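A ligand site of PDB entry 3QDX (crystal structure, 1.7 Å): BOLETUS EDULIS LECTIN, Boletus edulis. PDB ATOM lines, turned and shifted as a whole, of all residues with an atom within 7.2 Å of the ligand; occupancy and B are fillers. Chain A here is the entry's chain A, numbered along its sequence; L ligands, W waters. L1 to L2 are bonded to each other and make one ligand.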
ATOM      1  N   PHE A  27     -29.835  -1.247 -22.808  1.00  0.00           N
ATOM      2  CA  PHE A  27     -28.660  -0.525 -23.265  1.00  0.00           C
ATOM      3  C   PHE A  27     -27.941  -1.278 -24.428  1.00  0.00           C
ATOM      4  O   PHE A  27     -28.100  -2.500 -24.585  1.00  0.00           O
ATOM      5  CB  PHE A  27     -27.732  -0.216 -22.069  1.00  0.00           C
ATOM      6  CG  PHE A  27     -26.727   0.854 -22.363  1.00  0.00           C
ATOM      7  CD1 PHE A  27     -25.381   0.535 -22.459  1.00  0.00           C
ATOM      8  CD2 PHE A  27     -27.129   2.158 -22.569  1.00  0.00           C
ATOM      9  CE1 PHE A  27     -24.436   1.518 -22.761  1.00  0.00           C
ATOM     10  CE2 PHE A  27     -26.201   3.150 -22.856  1.00  0.00           C
ATOM     11  CZ  PHE A  27     -24.858   2.831 -22.961  1.00  0.00           C
ATOM     12  N   HIS A  28     -27.218  -0.525 -25.266  1.00  0.00           N
ATOM     13  CA  HIS A  28     -26.775  -1.000 -26.571  1.00  0.00           C
ATOM     14  C   HIS A  28     -25.430  -1.759 -26.581  1.00  0.00           C
ATOM     15  O   HIS A  28     -25.022  -2.287 -27.600  1.00  0.00           O
ATOM     16  CB  HIS A  28     -26.743   0.179 -27.568  1.00  0.00           C
ATOM     17  CG  HIS A  28     -25.655   1.181 -27.307  1.00  0.00           C
ATOM     18  ND1 HIS A  28     -25.852   2.321 -26.557  1.00  0.00           N
ATOM     19  CD2 HIS A  28     -24.376   1.221 -27.730  1.00  0.00           C
ATOM     20  CE1 HIS A  28     -24.727   3.007 -26.507  1.00  0.00           C
ATOM     21  NE2 HIS A  28     -23.809   2.353 -27.202  1.00  0.00           N
ATOM     22  N   TYR A  29     -24.733  -1.822 -25.448  1.00  0.00           N
ATOM     23  CA  TYR A  29     -23.490  -2.594 -25.423  1.00  0.00           C
ATOM     24  C   TYR A  29     -23.775  -4.103 -25.461  1.00  0.00           C
ATOM     25  O   TYR A  29     -24.902  -4.539 -25.228  1.00  0.00           O
ATOM     26  CB  TYR A  29     -22.738  -2.291 -24.141  1.00  0.00           C
ATOM     27  CG  TYR A  29     -22.047  -0.930 -24.063  1.00  0.00           C
ATOM     28  CD1 TYR A  29     -21.486  -0.505 -22.856  1.00  0.00           C
ATOM     29  CD2 TYR A  29     -21.972  -0.074 -25.160  1.00  0.00           C
ATOM     30  CE1 TYR A  29     -20.857   0.705 -22.744  1.00  0.00           C
ATOM     31  CE2 TYR A  29     -21.339   1.178 -25.048  1.00  0.00           C
ATOM     32  CZ  TYR A  29     -20.778   1.539 -23.842  1.00  0.00           C
ATOM     33  OH  TYR A  29     -20.126   2.762 -23.705  1.00  0.00           O
ATOM     34  N   ALA A  30     -22.740  -4.886 -25.735  1.00  0.00           N
ATOM     35  CA  ALA A  30     -22.818  -6.348 -25.638  1.00  0.00           C
ATOM     36  C   ALA A  30     -23.912  -6.897 -26.539  1.00  0.00           C
ATOM     37  O   ALA A  30     -24.586  -7.854 -26.192  1.00  0.00           O
ATOM     38  CB  ALA A  30     -23.034  -6.808 -24.190  1.00  0.00           C
ATOM     39  N   ASN A  31     -24.041  -6.294 -27.723  1.00  0.00           N
ATOM     40  CA  ASN A  31     -25.032  -6.724 -28.720  1.00  0.00           C
ATOM     41  C   ASN A  31     -26.485  -6.565 -28.239  1.00  0.00           C
ATOM     42  O   ASN A  31     -27.389  -7.235 -28.726  1.00  0.00           O
ATOM     43  CB  ASN A  31     -24.740  -8.142 -29.231  1.00  0.00           C
ATOM     44  CG  ASN A  31     -23.450  -8.204 -30.040  1.00  0.00           C
ATOM     45  OD1 ASN A  31     -23.227  -7.381 -30.916  1.00  0.00           O
ATOM     46  ND2 ASN A  31     -22.599  -9.154 -29.713  1.00  0.00           N
ATOM     47  N   GLY A  32     -26.673  -5.659 -27.289  1.00  0.00           N
ATOM     48  CA  GLY A  32     -28.016  -5.317 -26.812  1.00  0.00           C
ATOM     49  C   GLY A  32     -28.708  -6.462 -26.092  1.00  0.00           C
ATOM     50  O   GLY A  32     -28.106  -7.228 -25.329  1.00  0.00           O
ATOM     51  N   GLY A  47     -26.769  -9.986 -24.930  1.00  0.00           N
ATOM     52  CA  GLY A  47     -25.842 -10.649 -25.845  1.00  0.00           C
ATOM     53  C   GLY A  47     -24.505 -11.037 -25.259  1.00  0.00           C
ATOM     54  O   GLY A  47     -23.724 -11.737 -25.900  1.00  0.00           O
ATOM     55  N   GLY A  48     -24.231 -10.588 -24.031  1.00  0.00           N
ATOM     56  CA  GLY A  48     -22.970 -10.884 -23.372  1.00  0.00           C
ATOM     57  C   GLY A  48     -22.878 -10.129 -22.072  1.00  0.00           C
ATOM     58  O   GLY A  48     -23.852  -9.499 -21.652  1.00  0.00           O
ATOM     59  N   SER A  49     -21.721 -10.210 -21.405  1.00  0.00           N
ATOM     60  CA  SER A  49     -21.500  -9.345 -20.238  1.00  0.00           C
ATOM     61  C   SER A  49     -21.227  -7.915 -20.714  1.00  0.00           C
ATOM     62  O   SER A  49     -20.556  -7.727 -21.745  1.00  0.00           O
ATOM     63  CB  SER A  49     -20.301  -9.848 -19.403  1.00  0.00           C
ATOM     64  OG  SER A  49     -19.994  -8.941 -18.350  1.00  0.00           O
ATOM     65  N   GLY A  50     -21.755  -6.938 -19.976  1.00  0.00           N
ATOM     66  CA  GLY A  50     -21.386  -5.508 -20.156  1.00  0.00           C
ATOM     67  C   GLY A  50     -22.538  -4.603 -20.563  1.00  0.00           C
ATOM     68  O   GLY A  50     -22.329  -3.487 -21.038  1.00  0.00           O
ATOM     69  N   THR A  51     -23.760  -5.082 -20.430  1.00  0.00           N
ATOM     70  CA  THR A  51     -24.914  -4.247 -20.703  1.00  0.00           C
ATOM     71  C   THR A  51     -25.998  -4.429 -19.631  1.00  0.00           C
ATOM     72  O   THR A  51     -25.750  -5.049 -18.580  1.00  0.00           O
ATOM     73  CB  THR A  51     -25.460  -4.439 -22.137  1.00  0.00           C
ATOM     74  OG1 THR A  51     -26.287  -3.320 -22.487  1.00  0.00           O
ATOM     75  CG2 THR A  51     -26.286  -5.768 -22.263  1.00  0.00           C
ATOM     76  N   VAL A  71     -25.182  -7.070 -16.253  1.00  0.00           N
ATOM     77  CA  VAL A  71     -23.973  -7.810 -15.910  1.00  0.00           C
ATOM     78  C   VAL A  71     -22.749  -6.949 -16.222  1.00  0.00           C
ATOM     79  O   VAL A  71     -22.621  -6.417 -17.316  1.00  0.00           O
ATOM     80  CB  VAL A  71     -23.928  -9.150 -16.615  1.00  0.00           C
ATOM     81  CG1 VAL A  71     -22.673  -9.929 -16.160  1.00  0.00           C
ATOM     82  CG2 VAL A  71     -25.196  -9.957 -16.292  1.00  0.00           C
ATOM     83  N   HIS A  72     -21.865  -6.772 -15.244  1.00  0.00           N
ATOM     84  CA  HIS A  72     -20.649  -5.968 -15.452  1.00  0.00           C
ATOM     85  C   HIS A  72     -19.440  -6.842 -15.152  1.00  0.00           C
ATOM     86  O   HIS A  72     -19.306  -7.347 -14.040  1.00  0.00           O
ATOM     87  CB  HIS A  72     -20.630  -4.760 -14.507  1.00  0.00           C
ATOM     88  CG  HIS A  72     -19.362  -3.966 -14.594  1.00  0.00           C
ATOM     89  ND1 HIS A  72     -18.493  -3.823 -13.520  1.00  0.00           N
ATOM     90  CD2 HIS A  72     -18.792  -3.308 -15.632  1.00  0.00           C
ATOM     91  CE1 HIS A  72     -17.451  -3.082 -13.902  1.00  0.00           C
ATOM     92  NE2 HIS A  72     -17.619  -2.753 -15.173  1.00  0.00           N
ATOM     93  N   ASN A  73     -18.576  -7.018 -16.134  1.00  0.00           N
ATOM     94  CA  ASN A  73     -17.406  -7.882 -15.959  1.00  0.00           C
ATOM     95  C   ASN A  73     -17.773  -9.248 -15.355  1.00  0.00           C
ATOM     96  O   ASN A  73     -17.151  -9.737 -14.406  1.00  0.00           O
ATOM     97  CB  ASN A  73     -16.296  -7.151 -15.172  1.00  0.00           C
ATOM     98  CG  ASN A  73     -15.638  -6.038 -15.987  1.00  0.00           C
ATOM     99  OD1 ASN A  73     -15.685  -6.052 -17.213  1.00  0.00           O
ATOM    100  ND2 ASN A  73     -15.002  -5.082 -15.294  1.00  0.00           N
ATOM    101  N   TYR A  74     -18.800  -9.865 -15.944  1.00  0.00           N
ATOM    102  CA  TYR A  74     -19.231 -11.233 -15.624  1.00  0.00           C
ATOM    103  C   TYR A  74     -19.858 -11.395 -14.253  1.00  0.00           C
ATOM    104  O   TYR A  74     -20.040 -12.514 -13.784  1.00  0.00           O
ATOM    105  CB  TYR A  74     -18.067 -12.240 -15.830  1.00  0.00           C
ATOM    106  CG  TYR A  74     -17.373 -11.969 -17.144  1.00  0.00           C
ATOM    107  CD1 TYR A  74     -16.169 -11.291 -17.186  1.00  0.00           C
ATOM    108  CD2 TYR A  74     -17.970 -12.348 -18.341  1.00  0.00           C
ATOM    109  CE1 TYR A  74     -15.554 -11.013 -18.407  1.00  0.00           C
ATOM    110  CE2 TYR A  74     -17.349 -12.078 -19.565  1.00  0.00           C
ATOM    111  CZ  TYR A  74     -16.145 -11.407 -19.576  1.00  0.00           C
ATOM    112  OH  TYR A  74     -15.554 -11.127 -20.781  1.00  0.00           O
ATOM    113  N   LYS A  75     -20.213 -10.285 -13.597  1.00  0.00           N
ATOM    114  CA  LYS A  75     -20.931 -10.369 -12.326  1.00  0.00           C
ATOM    115  C   LYS A  75     -22.192  -9.525 -12.387  1.00  0.00           C
ATOM    116  O   LYS A  75     -22.176  -8.449 -12.979  1.00  0.00           O
ATOM    117  CB  LYS A  75     -20.063  -9.864 -11.173  1.00  0.00           C
ATOM    118  CG  LYS A  75     -18.782 -10.674 -10.952  1.00  0.00           C
ATOM    119  CD  LYS A  75     -18.116 -10.215  -9.688  1.00  0.00           C
ATOM    120  CE  LYS A  75     -16.799 -10.951  -9.495  1.00  0.00           C
ATOM    121  NZ  LYS A  75     -16.193 -10.607  -8.166  1.00  0.00           N
ATOM    122  N   TYR A  97     -25.635   5.053 -16.437  1.00  0.00           N
ATOM    123  CA  TYR A  97     -24.748   4.057 -15.831  1.00  0.00           C
ATOM    124  C   TYR A  97     -23.484   3.870 -16.646  1.00  0.00           C
ATOM    125  O   TYR A  97     -22.608   3.109 -16.251  1.00  0.00           O
ATOM    126  CB  TYR A  97     -25.474   2.721 -15.674  1.00  0.00           C
ATOM    127  CG  TYR A  97     -26.613   2.778 -14.696  1.00  0.00           C
ATOM    128  CD1 TYR A  97     -27.923   3.008 -15.127  1.00  0.00           C
ATOM    129  CD2 TYR A  97     -26.376   2.641 -13.335  1.00  0.00           C
ATOM    130  CE1 TYR A  97     -28.988   3.086 -14.209  1.00  0.00           C
ATOM    131  CE2 TYR A  97     -27.406   2.696 -12.416  1.00  0.00           C
ATOM    132  CZ  TYR A  97     -28.717   2.926 -12.847  1.00  0.00           C
ATOM    133  OH  TYR A  97     -29.712   3.006 -11.915  1.00  0.00           O
ATOM    134  N   TYR A  98     -23.383   4.560 -17.783  1.00  0.00           N
ATOM    135  CA  TYR A  98     -22.262   4.356 -18.697  1.00  0.00           C
ATOM    136  C   TYR A  98     -21.647   5.687 -19.116  1.00  0.00           C
ATOM    137  O   TYR A  98     -22.142   6.730 -18.735  1.00  0.00           O
ATOM    138  CB  TYR A  98     -22.727   3.597 -19.934  1.00  0.00           C
ATOM    139  CG  TYR A  98     -23.338   2.244 -19.579  1.00  0.00           C
ATOM    140  CD1 TYR A  98     -24.709   2.084 -19.362  1.00  0.00           C
ATOM    141  CD2 TYR A  98     -22.520   1.133 -19.412  1.00  0.00           C
ATOM    142  CE1 TYR A  98     -25.251   0.847 -19.032  1.00  0.00           C
ATOM    143  CE2 TYR A  98     -23.057  -0.127 -19.084  1.00  0.00           C
ATOM    144  CZ  TYR A  98     -24.419  -0.259 -18.899  1.00  0.00           C
ATOM    145  OH  TYR A  98     -24.951  -1.491 -18.561  1.00  0.00           O
ATOM    146  N   ASN A  99     -20.578   5.608 -19.900  1.00  0.00           N
ATOM    147  CA  ASN A  99     -19.885   6.790 -20.424  1.00  0.00           C
ATOM    148  C   ASN A  99     -19.554   7.815 -19.344  1.00  0.00           C
ATOM    149  O   ASN A  99     -19.761   9.024 -19.528  1.00  0.00           O
ATOM    150  CB  ASN A  99     -20.681   7.428 -21.564  1.00  0.00           C
ATOM    151  CG  ASN A  99     -20.837   6.479 -22.758  1.00  0.00           C
ATOM    152  OD1 ASN A  99     -19.879   6.247 -23.498  1.00  0.00           O
ATOM    153  ND2 ASN A  99     -22.027   5.912 -22.934  1.00  0.00           N
ATOM    154  N   ASN A 100     -19.059   7.301 -18.219  1.00  0.00           N
ATOM    155  CA  ASN A 100     -18.708   8.113 -17.045  1.00  0.00           C
ATOM    156  C   ASN A 100     -19.890   8.910 -16.487  1.00  0.00           C
ATOM    157  O   ASN A 100     -19.700   9.982 -15.897  1.00  0.00           O
ATOM    158  CB  ASN A 100     -17.525   9.034 -17.366  1.00  0.00           C
ATOM    159  CG  ASN A 100     -16.240   8.271 -17.640  1.00  0.00           C
ATOM    160  OD1 ASN A 100     -15.963   7.242 -17.006  1.00  0.00           O
ATOM    161  ND2 ASN A 100     -15.447   8.762 -18.583  1.00  0.00           N
ATOM    162  N   ALA A 104     -22.682   5.418 -12.829  1.00  0.00           N
ATOM    163  CA  ALA A 104     -21.746   4.316 -13.156  1.00  0.00           C
ATOM    164  C   ALA A 104     -21.195   3.648 -11.904  1.00  0.00           C
ATOM    165  O   ALA A 104     -20.985   2.424 -11.875  1.00  0.00           O
ATOM    166  CB  ALA A 104     -20.589   4.818 -14.045  1.00  0.00           C
ATOM    167  N   ARG A 107     -23.210   0.579 -10.877  1.00  0.00           N
ATOM    168  CA  ARG A 107     -22.941  -0.589 -11.708  1.00  0.00           C
ATOM    169  C   ARG A 107     -21.631  -1.259 -11.306  1.00  0.00           C
ATOM    170  O   ARG A 107     -21.529  -2.488 -11.240  1.00  0.00           O
ATOM    171  CB  ARG A 107     -22.933  -0.211 -13.198  1.00  0.00           C
ATOM    172  CG  ARG A 107     -22.305  -1.275 -14.117  1.00  0.00           C
ATOM    173  CD  ARG A 107     -22.393  -0.860 -15.593  1.00  0.00           C
ATOM    174  NE  ARG A 107     -21.748   0.433 -15.855  1.00  0.00           N
ATOM    175  CZ  ARG A 107     -20.429   0.640 -15.944  1.00  0.00           C
ATOM    176  NH1 ARG A 107     -19.574  -0.361 -15.785  1.00  0.00           N
ATOM    177  NH2 ARG A 107     -19.947   1.855 -16.157  1.00  0.00           N
ATOM    178  N   GLU A 108     -20.628  -0.427 -11.006  1.00  0.00           N
ATOM    179  CA  GLU A 108     -19.298  -0.943 -10.750  1.00  0.00           C
ATOM    180  C   GLU A 108     -19.243  -1.739  -9.448  1.00  0.00           C
ATOM    181  O   GLU A 108     -18.396  -2.619  -9.274  1.00  0.00           O
ATOM    182  CB  GLU A 108     -18.274   0.205 -10.790  1.00  0.00           C
ATOM    183  CG  GLU A 108     -18.018   0.704 -12.207  1.00  0.00           C
ATOM    184  CD  GLU A 108     -17.314   2.042 -12.276  1.00  0.00           C
ATOM    185  OE1 GLU A 108     -17.196   2.731 -11.231  1.00  0.00           O
ATOM    186  OE2 GLU A 108     -16.882   2.407 -13.388  1.00  0.00           O
HETATM  187  O1  LIG L   1     -17.775  -2.133 -18.526  1.00  0.00           O
HETATM  188  C1  LIG L   1     -17.087  -3.398 -18.793  1.00  0.00           C
HETATM  189  O2  LIG L   1     -15.712  -3.189 -19.216  1.00  0.00           O
HETATM  190  C2  LIG L   1     -17.891  -4.178 -19.833  1.00  0.00           C
HETATM  191  N1  LIG L   1     -17.240  -5.454 -20.184  1.00  0.00           N
HETATM  192  C3  LIG L   1     -18.098  -3.334 -21.085  1.00  0.00           C
HETATM  193  O3  LIG L   1     -18.949  -4.074 -21.947  1.00  0.00           O
HETATM  194  C4  LIG L   1     -18.763  -2.006 -20.719  1.00  0.00           C
HETATM  195  O4  LIG L   1     -20.059  -2.243 -20.121  1.00  0.00           O
HETATM  196  C5  LIG L   1     -17.919  -1.301 -19.671  1.00  0.00           C
HETATM  197  C6  LIG L   1     -18.663   0.026 -19.295  1.00  0.00           C
HETATM  198  O5  LIG L   1     -17.773   0.819 -18.473  1.00  0.00           O
HETATM  199  C7  LIG L   1     -17.698  -6.628 -19.719  1.00  0.00           C
HETATM  200  O6  LIG L   1     -18.664  -6.771 -18.974  1.00  0.00           O
HETATM  201  C8  LIG L   1     -16.900  -7.860 -20.199  1.00  0.00           C
HETATM  202  C1  LG2 L   2     -18.493  -4.159 -23.301  1.00  0.00           C
HETATM  203  C2  LG2 L   2     -19.314  -5.178 -24.093  1.00  0.00           C
HETATM  204  C3  LG2 L   2     -18.890  -5.105 -25.569  1.00  0.00           C
HETATM  205  C4  LG2 L   2     -19.025  -3.676 -26.066  1.00  0.00           C
HETATM  206  C5  LG2 L   2     -18.285  -2.713 -25.141  1.00  0.00           C
HETATM  207  C6  LG2 L   2     -18.580  -1.285 -25.578  1.00  0.00           C
HETATM  208  O1  LG2 L   2     -19.065  -6.467 -23.570  1.00  0.00           O
HETATM  209  O2  LG2 L   2     -19.641  -5.981 -26.397  1.00  0.00           O
HETATM  210  O3  LG2 L   2     -20.380  -3.235 -26.193  1.00  0.00           O
HETATM  211  O4  LG2 L   2     -18.694  -2.852 -23.784  1.00  0.00           O
HETATM  212  O5  LG2 L   2     -17.544  -0.470 -25.080  1.00  0.00           O
HETATM  213  O   HOH W   1     -20.868  -1.746 -28.487  1.00  0.00           O
HETATM  214  O   HOH W   2     -14.780  -5.313 -21.911  1.00  0.00           O
HETATM  215  O   HOH W   3     -16.970   0.527 -15.566  1.00  0.00           O
HETATM  216  O   HOH W   4     -16.565  -7.553 -24.113  1.00  0.00           O
HETATM  217  O   HOH W   5     -20.807  -3.137 -17.619  1.00  0.00           O
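The side-chain hydroxyl (OG) of Ser 49 sits at hydrogen-bond distance from the backbone NH (N) of Asn 73, at 3.3 Å. The backbone NH of Tyr 74 is in hydrogen-bond range of the side-chain hydroxyl of Ser 49 (2.8 Å). The backbone NH (N) of Gly 50 lies within hydrogen-bond range of the backbone carbonyl oxygen (O) of Val 71 (2.8 Å). O of Ala 30 lies close to N of Gly 47 (3.3 Å). The backbone carbonyl oxygen of Tyr 29 lies close to the side-chain hydroxyl of Thr 51, 3.3 Å away. A ring nitrogen (NE2) of His 72 sits close to the guanidinium group of Arg 107, 3.1 Å away. The backbone carbonyl oxygen (O) of Tyr 97 lies within hydrogen-bond range of the guanidinium group (NE) of Arg 107 (2.8 Å).
CB of Tyr 29 touches O3 of LG2 L2, at 3.3 Å. OH of Tyr 74 touches C8 of LIG L1, 3.6 Å away. CE2 of Tyr 98 touches O4 of LIG L1 (3.8 Å). Hydrophobic or aromatic side chains that line the ligand: Tyr 29, His 72, Tyr 74 and Tyr 98. Of the 23 residues printed, 9 come within 4 Å of the ligand. Along chain A the residues within 4 Å of the ligand span positions 29 to 107. The nearest printed residue that does not touch the ligand is Val 71 (4.3 Å).
Water W3 lies within hydrogen-bond range of the guanidinium group of Arg 107 (2.8 Å), the side-chain carboxylate of Glu 108 (2.9 Å), an oxygen (O5) of LIG L1 (3.0 Å) and a ring nitrogen (NE2) of His 72 (3.4 Å).
O1 of LG2 L2 is in hydrogen-bond range of O of Ser 49 (2.7 Å). OG of Ser 49 sits at hydrogen-bond distance from O6 of LIG L1 (2.6 Å). N of Gly 50 sits close to O6 of LIG L1, at 3.3 Å. O of Gly 50 sits at hydrogen-bond distance from O4 of LIG L1 (2.7 Å). The backbone NH of Asn 73 sits at hydrogen-bond distance from an oxygen (O6) of LIG L1. OD1 of Asn 73 lies close to N1 of LIG L1, at 3.4 Å. N of Ala 30 lies within hydrogen-bond range of O3 of LG2 L2. NE2 of His 72 sits close to O1 of LIG L1 (3.4 Å). The guanidinium group (NH2) of Arg 107 sits at hydrogen-bond distance from an oxygen (O5) of LIG L1, at 3.3 Å.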
